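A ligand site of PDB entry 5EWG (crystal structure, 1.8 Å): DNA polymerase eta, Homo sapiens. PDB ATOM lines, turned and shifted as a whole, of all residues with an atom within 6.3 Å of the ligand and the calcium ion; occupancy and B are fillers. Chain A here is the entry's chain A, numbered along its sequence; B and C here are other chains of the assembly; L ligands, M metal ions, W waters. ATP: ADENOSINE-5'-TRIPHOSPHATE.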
ATOM      1  N   ASP A  16      27.961 -22.883  16.382  1.00  0.00           N
ATOM      2  CA  ASP A  16      28.105 -23.745  15.207  1.00  0.00           C
ATOM      3  C   ASP A  16      27.804 -25.187  15.625  1.00  0.00           C
ATOM      4  O   ASP A  16      28.529 -25.738  16.446  1.00  0.00           O
ATOM      5  CB  ASP A  16      29.531 -23.615  14.655  1.00  0.00           C
ATOM      6  CG  ASP A  16      29.726 -24.250  13.305  1.00  0.00           C
ATOM      7  OD1 ASP A  16      29.062 -25.226  13.015  1.00  0.00           O
ATOM      8  OD2 ASP A  16      30.564 -23.749  12.514  1.00  0.00           O
ATOM      9  N   MET A  17      26.772 -25.792  15.047  1.00  0.00           N
ATOM     10  CA  MET A  17      26.456 -27.166  15.452  1.00  0.00           C
ATOM     11  C   MET A  17      27.546 -28.126  14.994  1.00  0.00           C
ATOM     12  O   MET A  17      28.050 -28.041  13.881  1.00  0.00           O
ATOM     13  CB  MET A  17      25.096 -27.604  14.889  1.00  0.00           C
ATOM     14  CG  MET A  17      23.953 -26.639  15.175  1.00  0.00           C
ATOM     15  SD  MET A  17      23.752 -26.313  16.927  1.00  0.00           S
ATOM     16  CE  MET A  17      23.323 -27.915  17.579  1.00  0.00           C
ATOM     17  N   ASP A  18      27.952 -29.048  15.874  1.00  0.00           N
ATOM     18  CA  ASP A  18      28.956 -30.038  15.490  1.00  0.00           C
ATOM     19  C   ASP A  18      28.332 -31.074  14.562  1.00  0.00           C
ATOM     20  O   ASP A  18      27.220 -31.533  14.802  1.00  0.00           O
ATOM     21  CB  ASP A  18      29.551 -30.729  16.724  1.00  0.00           C
ATOM     22  CG  ASP A  18      30.232 -29.741  17.669  1.00  0.00           C
ATOM     23  OD1 ASP A  18      30.836 -28.772  17.189  1.00  0.00           O
ATOM     24  OD2 ASP A  18      30.164 -29.949  18.899  1.00  0.00           O
ATOM     25  N   CYS A  19      29.071 -31.444  13.503  1.00  0.00           N
ATOM     26  CA  CYS A  19      28.651 -32.399  12.460  1.00  0.00           C
ATOM     27  C   CYS A  19      27.132 -32.530  12.381  1.00  0.00           C
ATOM     28  O   CYS A  19      26.573 -33.598  12.685  1.00  0.00           O
ATOM     29  CB  CYS A  19      29.308 -33.765  12.685  1.00  0.00           C
ATOM     30  SG  CYS A  19      29.206 -34.479  14.352  1.00  0.00           S
ATOM     31  N   PHE A  20      26.470 -31.458  11.966  1.00  0.00           N
ATOM     32  CA  PHE A  20      25.056 -31.245  12.283  1.00  0.00           C
ATOM     33  C   PHE A  20      24.171 -32.364  11.725  1.00  0.00           C
ATOM     34  O   PHE A  20      23.349 -32.931  12.465  1.00  0.00           O
ATOM     35  CB  PHE A  20      24.590 -29.899  11.739  1.00  0.00           C
ATOM     36  CG  PHE A  20      23.156 -29.597  12.061  1.00  0.00           C
ATOM     37  CD1 PHE A  20      22.696 -29.739  13.363  1.00  0.00           C
ATOM     38  CD2 PHE A  20      22.278 -29.175  11.076  1.00  0.00           C
ATOM     39  CE1 PHE A  20      21.362 -29.471  13.684  1.00  0.00           C
ATOM     40  CE2 PHE A  20      20.948 -28.900  11.390  1.00  0.00           C
ATOM     41  CZ  PHE A  20      20.491 -29.051  12.683  1.00  0.00           C
ATOM     42  N   PHE A  21      24.266 -32.656  10.425  1.00  0.00           N
ATOM     43  CA  PHE A  21      23.369 -33.670   9.847  1.00  0.00           C
ATOM     44  C   PHE A  21      23.592 -35.031  10.508  1.00  0.00           C
ATOM     45  O   PHE A  21      22.649 -35.823  10.691  1.00  0.00           O
ATOM     46  CB  PHE A  21      23.584 -33.800   8.328  1.00  0.00           C
ATOM     47  CG  PHE A  21      23.030 -32.650   7.495  1.00  0.00           C
ATOM     48  CD1 PHE A  21      22.709 -31.434   8.050  1.00  0.00           C
ATOM     49  CD2 PHE A  21      22.858 -32.825   6.124  1.00  0.00           C
ATOM     50  CE1 PHE A  21      22.212 -30.402   7.254  1.00  0.00           C
ATOM     51  CE2 PHE A  21      22.361 -31.814   5.338  1.00  0.00           C
ATOM     52  CZ  PHE A  21      22.044 -30.593   5.901  1.00  0.00           C
ATOM     53  N   VAL A  22      24.847 -35.336  10.869  1.00  0.00           N
ATOM     54  CA  VAL A  22      25.154 -36.568  11.594  1.00  0.00           C
ATOM     55  C   VAL A  22      24.435 -36.597  12.947  1.00  0.00           C
ATOM     56  O   VAL A  22      23.823 -37.602  13.324  1.00  0.00           O
ATOM     57  CB  VAL A  22      26.672 -36.730  11.765  1.00  0.00           C
ATOM     58  CG1 VAL A  22      26.994 -37.873  12.749  1.00  0.00           C
ATOM     59  CG2 VAL A  22      27.349 -36.980  10.422  1.00  0.00           C
ATOM     60  N   GLN A  41      24.260 -38.233   0.255  1.00  0.00           N
ATOM     61  CA  GLN A  41      23.249 -37.718  -0.665  1.00  0.00           C
ATOM     62  C   GLN A  41      23.293 -38.574  -1.925  1.00  0.00           C
ATOM     63  O   GLN A  41      24.355 -38.732  -2.520  1.00  0.00           O
ATOM     64  CB  GLN A  41      23.545 -36.255  -0.991  1.00  0.00           C
ATOM     65  CG  GLN A  41      22.375 -35.359  -1.177  1.00  0.00           C
ATOM     66  CD  GLN A  41      22.747 -33.909  -0.906  1.00  0.00           C
ATOM     67  OE1 GLN A  41      21.966 -33.152  -0.345  1.00  0.00           O
ATOM     68  NE2 GLN A  41      23.963 -33.529  -1.288  1.00  0.00           N
ATOM     69  N   ILE A  51      27.977 -35.716   2.680  1.00  0.00           N
ATOM     70  CA  ILE A  51      27.682 -34.329   3.027  1.00  0.00           C
ATOM     71  C   ILE A  51      28.035 -33.988   4.490  1.00  0.00           C
ATOM     72  O   ILE A  51      28.189 -32.802   4.799  1.00  0.00           O
ATOM     73  CB  ILE A  51      26.205 -33.994   2.712  1.00  0.00           C
ATOM     74  CG1 ILE A  51      25.877 -32.512   2.907  1.00  0.00           C
ATOM     75  CG2 ILE A  51      25.241 -34.866   3.516  1.00  0.00           C
ATOM     76  CD1 ILE A  51      26.579 -31.616   1.888  1.00  0.00           C
ATOM     77  N   ALA A  52      28.176 -34.975   5.374  1.00  0.00           N
ATOM     78  CA  ALA A  52      28.535 -34.728   6.780  1.00  0.00           C
ATOM     79  C   ALA A  52      29.199 -35.957   7.370  1.00  0.00           C
ATOM     80  O   ALA A  52      28.850 -37.088   7.018  1.00  0.00           O
ATOM     81  CB  ALA A  52      27.305 -34.335   7.628  1.00  0.00           C
ATOM     82  N   VAL A  53      30.134 -35.735   8.297  1.00  0.00           N
ATOM     83  CA  VAL A  53      31.019 -36.784   8.800  1.00  0.00           C
ATOM     84  C   VAL A  53      31.172 -36.669  10.310  1.00  0.00           C
ATOM     85  O   VAL A  53      31.554 -35.596  10.808  1.00  0.00           O
ATOM     86  CB  VAL A  53      32.412 -36.706   8.144  1.00  0.00           C
ATOM     87  CG1 VAL A  53      33.269 -37.903   8.549  1.00  0.00           C
ATOM     88  CG2 VAL A  53      32.314 -36.602   6.647  1.00  0.00           C
ATOM     89  N   TYR A  55      32.917 -37.117  14.017  1.00  0.00           N
ATOM     90  CA  TYR A  55      34.322 -36.938  14.384  1.00  0.00           C
ATOM     91  C   TYR A  55      35.067 -38.268  14.456  1.00  0.00           C
ATOM     92  O   TYR A  55      36.241 -38.334  14.090  1.00  0.00           O
ATOM     93  CB  TYR A  55      34.436 -36.137  15.694  1.00  0.00           C
ATOM     94  CG  TYR A  55      34.253 -34.651  15.424  1.00  0.00           C
ATOM     95  CD1 TYR A  55      32.982 -34.121  15.223  1.00  0.00           C
ATOM     96  CD2 TYR A  55      35.334 -33.805  15.286  1.00  0.00           C
ATOM     97  CE1 TYR A  55      32.796 -32.767  14.930  1.00  0.00           C
ATOM     98  CE2 TYR A  55      35.178 -32.448  15.001  1.00  0.00           C
ATOM     99  CZ  TYR A  55      33.898 -31.932  14.811  1.00  0.00           C
ATOM    100  OH  TYR A  55      33.704 -30.589  14.516  1.00  0.00           O
ATOM    101  N   ARG A  58      36.074 -38.895  10.906  1.00  0.00           N
ATOM    102  CA  ARG A  58      37.106 -37.965  10.433  1.00  0.00           C
ATOM    103  C   ARG A  58      38.500 -38.452  10.780  1.00  0.00           C
ATOM    104  O   ARG A  58      39.449 -38.184  10.028  1.00  0.00           O
ATOM    105  CB  ARG A  58      36.882 -36.575  11.012  1.00  0.00           C
ATOM    106  CG  ARG A  58      35.540 -35.977  10.631  1.00  0.00           C
ATOM    107  CD  ARG A  58      35.378 -34.564  11.177  1.00  0.00           C
ATOM    108  NE  ARG A  58      33.993 -34.138  10.991  1.00  0.00           N
ATOM    109  CZ  ARG A  58      33.549 -32.899  11.205  1.00  0.00           C
ATOM    110  NH1 ARG A  58      34.391 -31.947  11.596  1.00  0.00           N
ATOM    111  NH2 ARG A  58      32.276 -32.623  11.004  1.00  0.00           N
ATOM    112  N   ARG A  64      33.724 -34.460   3.766  1.00  0.00           N
ATOM    113  CA  ARG A  64      32.666 -34.000   2.886  1.00  0.00           C
ATOM    114  C   ARG A  64      33.159 -33.981   1.440  1.00  0.00           C
ATOM    115  O   ARG A  64      34.345 -33.786   1.176  1.00  0.00           O
ATOM    116  CB  ARG A  64      32.186 -32.616   3.337  1.00  0.00           C
ATOM    117  CG  ARG A  64      31.413 -31.792   2.310  1.00  0.00           C
ATOM    118  CD  ARG A  64      30.872 -30.498   2.937  1.00  0.00           C
ATOM    119  NE  ARG A  64      30.022 -30.801   4.085  1.00  0.00           N
ATOM    120  CZ  ARG A  64      30.186 -30.314   5.309  1.00  0.00           C
ATOM    121  NH1 ARG A  64      31.160 -29.439   5.564  1.00  0.00           N
ATOM    122  NH2 ARG A  64      29.362 -30.673   6.284  1.00  0.00           N
ATOM    123  N   LEU A  92      16.066 -31.701   2.154  1.00  0.00           N
ATOM    124  CA  LEU A  92      16.756 -31.381   3.405  1.00  0.00           C
ATOM    125  C   LEU A  92      15.803 -30.954   4.517  1.00  0.00           C
ATOM    126  O   LEU A  92      16.251 -30.389   5.522  1.00  0.00           O
ATOM    127  CB  LEU A  92      17.791 -30.280   3.145  1.00  0.00           C
ATOM    128  CG  LEU A  92      18.793 -30.589   2.023  1.00  0.00           C
ATOM    129  CD1 LEU A  92      19.816 -29.467   1.883  1.00  0.00           C
ATOM    130  CD2 LEU A  92      19.471 -31.902   2.347  1.00  0.00           C
ATOM    131  N   SER A 116      23.727 -19.722   8.578  1.00  0.00           N
ATOM    132  CA  SER A 116      23.630 -20.900   7.726  1.00  0.00           C
ATOM    133  C   SER A 116      22.587 -21.815   8.347  1.00  0.00           C
ATOM    134  O   SER A 116      21.959 -21.465   9.342  1.00  0.00           O
ATOM    135  CB  SER A 116      24.980 -21.615   7.601  1.00  0.00           C
ATOM    136  OG  SER A 116      25.343 -22.180   8.853  1.00  0.00           O
ATOM    137  N   ILE A 117      22.405 -23.000   7.756  1.00  0.00           N
ATOM    138  CA  ILE A 117      21.462 -23.943   8.348  1.00  0.00           C
ATOM    139  C   ILE A 117      21.859 -24.308   9.782  1.00  0.00           C
ATOM    140  O   ILE A 117      21.003 -24.636  10.598  1.00  0.00           O
ATOM    141  CB  ILE A 117      21.332 -25.209   7.469  1.00  0.00           C
ATOM    142  CG1 ILE A 117      20.168 -26.078   7.936  1.00  0.00           C
ATOM    143  CG2 ILE A 117      22.636 -26.014   7.463  1.00  0.00           C
ATOM    144  CD1 ILE A 117      19.805 -27.170   6.941  1.00  0.00           C
ATOM    145  N   ASP A 118      23.155 -24.204  10.133  1.00  0.00           N
ATOM    146  CA  ASP A 118      23.550 -24.648  11.470  1.00  0.00           C
ATOM    147  C   ASP A 118      24.474 -23.667  12.185  1.00  0.00           C
ATOM    148  O   ASP A 118      25.160 -24.051  13.146  1.00  0.00           O
ATOM    149  CB  ASP A 118      24.191 -26.027  11.387  1.00  0.00           C
ATOM    150  CG  ASP A 118      25.642 -25.964  10.966  1.00  0.00           C
ATOM    151  OD1 ASP A 118      25.997 -25.088  10.136  1.00  0.00           O
ATOM    152  OD2 ASP A 118      26.427 -26.781  11.487  1.00  0.00           O
ATOM    153  N   GLU A 119      24.503 -22.404  11.781  1.00  0.00           N
ATOM    154  CA  GLU A 119      25.269 -21.378  12.486  1.00  0.00           C
ATOM    155  C   GLU A 119      24.405 -20.151  12.741  1.00  0.00           C
ATOM    156  O   GLU A 119      23.587 -19.768  11.890  1.00  0.00           O
ATOM    157  CB  GLU A 119      26.514 -20.945  11.702  1.00  0.00           C
ATOM    158  CG  GLU A 119      27.588 -21.988  11.566  1.00  0.00           C
ATOM    159  CD  GLU A 119      28.802 -21.437  10.816  1.00  0.00           C
ATOM    160  OE1 GLU A 119      28.764 -20.241  10.456  1.00  0.00           O
ATOM    161  OE2 GLU A 119      29.771 -22.174  10.576  1.00  0.00           O
ATOM    162  N   LYS A 234      37.030 -27.558  18.608  1.00  0.00           N
ATOM    163  CA  LYS A 234      35.848 -28.335  18.196  1.00  0.00           C
ATOM    164  C   LYS A 234      36.171 -29.803  18.469  1.00  0.00           C
ATOM    165  O   LYS A 234      37.347 -30.190  18.392  1.00  0.00           O
ATOM    166  CB  LYS A 234      35.514 -28.109  16.708  1.00  0.00           C
ATOM    167  CG  LYS A 234      34.488 -27.004  16.379  1.00  0.00           C
ATOM    168  CD  LYS A 234      33.851 -27.248  14.964  1.00  0.00           C
ATOM    169  CE  LYS A 234      32.526 -26.486  14.693  1.00  0.00           C
ATOM    170  NZ  LYS A 234      31.235 -27.153  15.156  1.00  0.00           N
ATOM    171  N   PRO A 235      35.165 -30.629  18.791  1.00  0.00           N
ATOM    172  CA  PRO A 235      33.747 -30.322  18.976  1.00  0.00           C
ATOM    173  C   PRO A 235      33.383 -30.107  20.437  1.00  0.00           C
ATOM    174  O   PRO A 235      34.200 -30.366  21.316  1.00  0.00           O
ATOM    175  CB  PRO A 235      33.058 -31.575  18.450  1.00  0.00           C
ATOM    176  CG  PRO A 235      34.009 -32.692  18.901  1.00  0.00           C
ATOM    177  CD  PRO A 235      35.410 -32.082  18.850  1.00  0.00           C
ATOM    178  P    DT B   3      33.443 -34.815  -9.512  1.00  0.00           P
ATOM    179  OP1  DT B   3      34.343 -34.518 -10.648  1.00  0.00           O
ATOM    180  OP2  DT B   3      33.991 -35.372  -8.255  1.00  0.00           O
ATOM    181  O5'  DT B   3      32.627 -33.473  -9.203  1.00  0.00           O
ATOM    182  C5'  DT B   3      32.197 -33.176  -7.883  1.00  0.00           C
ATOM    183  C4'  DT B   3      30.866 -33.842  -7.570  1.00  0.00           C
ATOM    184  O4'  DT B   3      30.675 -33.879  -6.133  1.00  0.00           O
ATOM    185  C3'  DT B   3      29.643 -33.125  -8.136  1.00  0.00           C
ATOM    186  O3'  DT B   3      28.589 -34.075  -8.385  1.00  0.00           O
ATOM    187  C2'  DT B   3      29.288 -32.181  -6.997  1.00  0.00           C
ATOM    188  C1'  DT B   3      29.590 -33.037  -5.781  1.00  0.00           C
ATOM    189  N1   DT B   3      29.979 -32.254  -4.551  1.00  0.00           N
ATOM    190  C2   DT B   3      29.300 -32.469  -3.379  1.00  0.00           C
ATOM    191  O2   DT B   3      28.384 -33.259  -3.260  1.00  0.00           O
ATOM    192  N3   DT B   3      29.737 -31.714  -2.323  1.00  0.00           N
ATOM    193  C4   DT B   3      30.764 -30.791  -2.319  1.00  0.00           C
ATOM    194  O4   DT B   3      31.076 -30.155  -1.310  1.00  0.00           O
ATOM    195  C5   DT B   3      31.439 -30.607  -3.586  1.00  0.00           C
ATOM    196  C7   DT B   3      32.575 -29.625  -3.708  1.00  0.00           C
ATOM    197  C6   DT B   3      31.015 -31.348  -4.631  1.00  0.00           C
ATOM    198  P   8OG B   4      27.163 -33.609  -8.954  1.00  0.00           P
ATOM    199  OP1 8OG B   4      26.439 -34.861  -9.400  1.00  0.00           O
ATOM    200  OP2 8OG B   4      27.339 -32.441  -9.889  1.00  0.00           O
ATOM    201  O5' 8OG B   4      26.383 -33.068  -7.645  1.00  0.00           O
ATOM    202  C5' 8OG B   4      25.941 -34.000  -6.652  1.00  0.00           C
ATOM    203  C4' 8OG B   4      25.218 -33.229  -5.561  1.00  0.00           C
ATOM    204  O4' 8OG B   4      26.137 -32.558  -4.706  1.00  0.00           O
ATOM    205  C3' 8OG B   4      24.305 -32.143  -6.092  1.00  0.00           C
ATOM    206  O3' 8OG B   4      23.038 -32.404  -5.515  1.00  0.00           O
ATOM    207  C2' 8OG B   4      24.778 -30.845  -5.479  1.00  0.00           C
ATOM    208  C1' 8OG B   4      25.518 -31.355  -4.265  1.00  0.00           C
ATOM    209  N9  8OG B   4      26.533 -30.389  -3.816  1.00  0.00           N
ATOM    210  C8  8OG B   4      26.702 -30.005  -2.557  1.00  0.00           C
ATOM    211  N7  8OG B   4      27.680 -29.113  -2.349  1.00  0.00           N
ATOM    212  C5  8OG B   4      28.190 -28.892  -3.568  1.00  0.00           C
ATOM    213  C6  8OG B   4      29.273 -28.042  -4.118  1.00  0.00           C
ATOM    214  O6  8OG B   4      29.947 -27.319  -3.363  1.00  0.00           O
ATOM    215  N1  8OG B   4      29.497 -28.074  -5.441  1.00  0.00           N
ATOM    216  C2  8OG B   4      28.783 -28.846  -6.286  1.00  0.00           C
ATOM    217  N2  8OG B   4      29.099 -28.806  -7.609  1.00  0.00           N
ATOM    218  N3  8OG B   4      27.776 -29.650  -5.850  1.00  0.00           N
ATOM    219  C4  8OG B   4      27.438 -29.716  -4.541  1.00  0.00           C
ATOM    220  O8  8OG B   4      25.958 -30.484  -1.617  1.00  0.00           O
ATOM    221  P    DA B   5      21.780 -31.473  -5.843  1.00  0.00           P
ATOM    222  OP1  DA B   5      20.592 -32.371  -5.795  1.00  0.00           O
ATOM    223  OP2  DA B   5      22.086 -30.654  -7.040  1.00  0.00           O
ATOM    224  O5'  DA B   5      21.674 -30.515  -4.574  1.00  0.00           O
ATOM    225  C5'  DA B   5      21.303 -31.065  -3.322  1.00  0.00           C
ATOM    226  C4'  DA B   5      21.004 -29.960  -2.328  1.00  0.00           C
ATOM    227  O4'  DA B   5      22.230 -29.280  -1.969  1.00  0.00           O
ATOM    228  C3'  DA B   5      20.034 -28.892  -2.819  1.00  0.00           C
ATOM    229  O3'  DA B   5      19.096 -28.656  -1.808  1.00  0.00           O
ATOM    230  C2'  DA B   5      20.940 -27.663  -3.070  1.00  0.00           C
ATOM    231  C1'  DA B   5      22.043 -27.899  -2.038  1.00  0.00           C
ATOM    232  N9   DA B   5      23.338 -27.310  -2.367  1.00  0.00           N
ATOM    233  C8   DA B   5      24.040 -27.434  -3.537  1.00  0.00           C
ATOM    234  N7   DA B   5      25.205 -26.835  -3.514  1.00  0.00           N
ATOM    235  C5   DA B   5      25.279 -26.296  -2.241  1.00  0.00           C
ATOM    236  C6   DA B   5      26.266 -25.540  -1.563  1.00  0.00           C
ATOM    237  N6   DA B   5      27.416 -25.170  -2.128  1.00  0.00           N
ATOM    238  N1   DA B   5      26.018 -25.176  -0.288  1.00  0.00           N
ATOM    239  C2   DA B   5      24.861 -25.541   0.278  1.00  0.00           C
ATOM    240  N3   DA B   5      23.870 -26.251  -0.258  1.00  0.00           N
ATOM    241  C4   DA B   5      24.144 -26.602  -1.517  1.00  0.00           C
ATOM    242  P    DT C   8      32.439 -21.547   6.037  1.00  0.00           P
ATOM    243  OP1  DT C   8      33.112 -21.485   7.360  1.00  0.00           O
ATOM    244  OP2  DT C   8      32.999 -22.404   4.964  1.00  0.00           O
ATOM    245  O5'  DT C   8      30.937 -22.048   6.251  1.00  0.00           O
ATOM    246  C5'  DT C   8      30.006 -21.242   6.970  1.00  0.00           C
ATOM    247  C4'  DT C   8      28.669 -21.939   7.101  1.00  0.00           C
ATOM    248  O4'  DT C   8      28.079 -22.097   5.792  1.00  0.00           O
ATOM    249  C3'  DT C   8      28.726 -23.341   7.712  1.00  0.00           C
ATOM    250  O3'  DT C   8      27.564 -23.552   8.516  1.00  0.00           O
ATOM    251  C2'  DT C   8      28.748 -24.252   6.491  1.00  0.00           C
ATOM    252  C1'  DT C   8      27.901 -23.465   5.485  1.00  0.00           C
ATOM    253  N1   DT C   8      28.283 -23.668   4.070  1.00  0.00           N
ATOM    254  C2   DT C   8      27.307 -23.997   3.156  1.00  0.00           C
ATOM    255  O2   DT C   8      26.136 -24.146   3.452  1.00  0.00           O
ATOM    256  N3   DT C   8      27.755 -24.161   1.872  1.00  0.00           N
ATOM    257  C4   DT C   8      29.046 -24.016   1.413  1.00  0.00           C
ATOM    258  O4   DT C   8      29.349 -24.179   0.233  1.00  0.00           O
ATOM    259  C5   DT C   8      30.021 -23.659   2.414  1.00  0.00           C
ATOM    260  C7   DT C   8      31.461 -23.485   2.032  1.00  0.00           C
ATOM    261  C6   DT C   8      29.601 -23.506   3.688  1.00  0.00           C
HETATM  262  PG  ATP L   1      31.533 -29.208  11.882  1.00  0.00           P
HETATM  263  O1G ATP L   1      32.945 -29.127  11.313  1.00  0.00           O
HETATM  264  O2G ATP L   1      31.467 -29.995  13.155  1.00  0.00           O
HETATM  265  O3G ATP L   1      30.764 -27.909  11.875  1.00  0.00           O
HETATM  266  PB  ATP L   1      29.380 -29.877  10.031  1.00  0.00           P
HETATM  267  O1B ATP L   1      28.972 -31.173   9.346  1.00  0.00           O
HETATM  268  O2B ATP L   1      28.373 -29.141  10.887  1.00  0.00           O
HETATM  269  O3B ATP L   1      30.765 -30.163  10.808  1.00  0.00           O
HETATM  270  PA  ATP L   1      29.587 -27.430   8.435  1.00  0.00           P
HETATM  271  O1A ATP L   1      30.731 -27.001   7.535  1.00  0.00           O
HETATM  272  O2A ATP L   1      29.229 -26.608   9.648  1.00  0.00           O
HETATM  273  O3A ATP L   1      29.918 -28.963   8.808  1.00  0.00           O
HETATM  274  O5' ATP L   1      28.278 -27.517   7.536  1.00  0.00           O
HETATM  275  C5' ATP L   1      26.955 -27.402   8.061  1.00  0.00           C
HETATM  276  C4' ATP L   1      26.002 -27.623   6.895  1.00  0.00           C
HETATM  277  O4' ATP L   1      26.253 -26.653   5.878  1.00  0.00           O
HETATM  278  C3' ATP L   1      26.163 -28.964   6.191  1.00  0.00           C
HETATM  279  O3' ATP L   1      25.380 -29.999   6.788  1.00  0.00           O
HETATM  280  C2' ATP L   1      25.659 -28.670   4.801  1.00  0.00           C
HETATM  281  O2' ATP L   1      24.235 -28.716   4.827  1.00  0.00           O
HETATM  282  C1' ATP L   1      26.031 -27.217   4.587  1.00  0.00           C
HETATM  283  N9  ATP L   1      27.296 -27.217   3.828  1.00  0.00           N
HETATM  284  C8  ATP L   1      28.549 -26.904   4.263  1.00  0.00           C
HETATM  285  N7  ATP L   1      29.451 -27.037   3.248  1.00  0.00           N
HETATM  286  C5  ATP L   1      28.758 -27.433   2.147  1.00  0.00           C
HETATM  287  C6  ATP L   1      29.061 -27.757   0.735  1.00  0.00           C
HETATM  288  N6  ATP L   1      30.328 -27.691   0.266  1.00  0.00           N
HETATM  289  N1  ATP L   1      28.041 -28.142  -0.054  1.00  0.00           N
HETATM  290  C2  ATP L   1      26.778 -28.234   0.401  1.00  0.00           C
HETATM  291  N3  ATP L   1      26.411 -27.955   1.659  1.00  0.00           N
HETATM  292  C4  ATP L   1      27.349 -27.553   2.547  1.00  0.00           C
HETATM  293 CA    CA M   1      28.695 -27.102  11.843  1.00  0.00          CA
HETATM  294  O   HOH W   1      30.702 -32.987   8.576  1.00  0.00           O
HETATM  295  O   HOH W   2      23.625 -28.912   2.269  1.00  0.00           O
HETATM  296  O   HOH W   3      26.164 -31.413   8.777  1.00  0.00           O
HETATM  297  O   HOH W   4      33.733 -29.480   8.879  1.00  0.00           O
HETATM  298  O   HOH W   5      31.654 -24.981  10.500  1.00  0.00           O
HETATM  299  O   HOH W   6      33.062 -27.258   1.228  1.00  0.00           O
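N7 of 8OG 4 of chain B lies close to N1 of the ligand (2.5 Å). The side-chain hydroxyl (OH) of Tyr 55 sits at hydrogen-bond distance from an oxygen (O2G) of the ligand, at 2.7 Å. An oxygen (O2G) of the ligand sits at hydrogen-bond distance from the backbone NH (N) of Cys 19 (2.8 Å). An oxygen (O1G) of the ligand is in salt-bridge range of the guanidinium group (NH1) of Arg 58, 3.2 Å away. O4 of DT 3 of chain B is in hydrogen-bond range of a nitrogen (N6) of the ligand. The guanidinium group (NH2) of Arg 64 lies within salt-bridge range of an oxygen (O1B) of the ligand (3.1 Å). An oxygen (O2B) of the ligand lies close to the backbone NH (N) of Phe 20, 3.2 Å away. An oxygen (O2G) of the ligand lies within salt-bridge range of the side-chain amino group (NZ) of Lys 234 (3.5 Å).
NZ of Lys 234 is in hydrogen-bond range of O of Asp 16, at 3.3 Å. The side-chain carboxylate of Glu 119 sits close to the side-chain carboxylate of Asp 16, at 2.6 Å. O3' of DT 8 of chain C sits close to the side-chain carboxylate of Asp 118, 2.7 Å away. OH of Tyr 55 lies close to NH1 of Arg 58 (3.3 Å). NE of Arg 58 is in hydrogen-bond range of O of Val 53. The guanidinium group of Arg 64 sits at hydrogen-bond distance from the backbone carbonyl oxygen of Ile 51 (2.8 Å). The side-chain hydroxyl of Ser 116 is in hydrogen-bond range of O3' of DT 8 of chain C (2.6 Å). NZ of Lys 234 is in salt-bridge range of OD1 of Asp 18.
N3 of the ligand lies close to N1 of DA 5 of chain B (3.4 Å). O2 of DT 8 of chain C lies close to a nitrogen (N9) of the ligand (3.3 Å). Residues that only touch the ligand: Phe 21 (3.1 Å), Asp 18 (3.4 Å), Ile 51 (3.7 Å), Ile 117 (3.8 Å) and Ala 52 (3.97 Å). Hydrophobic or aromatic side chains that line the ligand: Phe 20, Phe 21, Ile 51, Ala 52, Tyr 55 and Ile 117. Of the 25 residues printed, 18 come within 4 Å of the ligand.
Within 4 Å of the calcium ion: Asp 16, Met 17 and Asp 118. The nearest printed residue that does not touch the calcium ion is Lys 234 (4.2 Å).
The calcium ion is bound by O3G of the ligand (2.2 Å), OD1 of Asp 16 (2.2 Å), O2B of the ligand (2.3 Å), O2A of the ligand (2.3 Å), OD2 of Asp 118 (2.3 Å) and O of Met 17 (2.3 Å).
Water W3 lies within hydrogen-bond range of O3' of the ligand (2.6 Å), N of Phe 21 (2.8 Å) and N of Phe 20 (3.2 Å). Water W1 lies within hydrogen-bond range of an oxygen (O1B) of the ligand, the backbone NH of Val 53 and the guanidinium group of Arg 58. Water W5 lies within hydrogen-bond range of the side-chain carboxylate (OD2) of Asp 16 and the side-chain carboxylate (OE2) of Glu 119.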
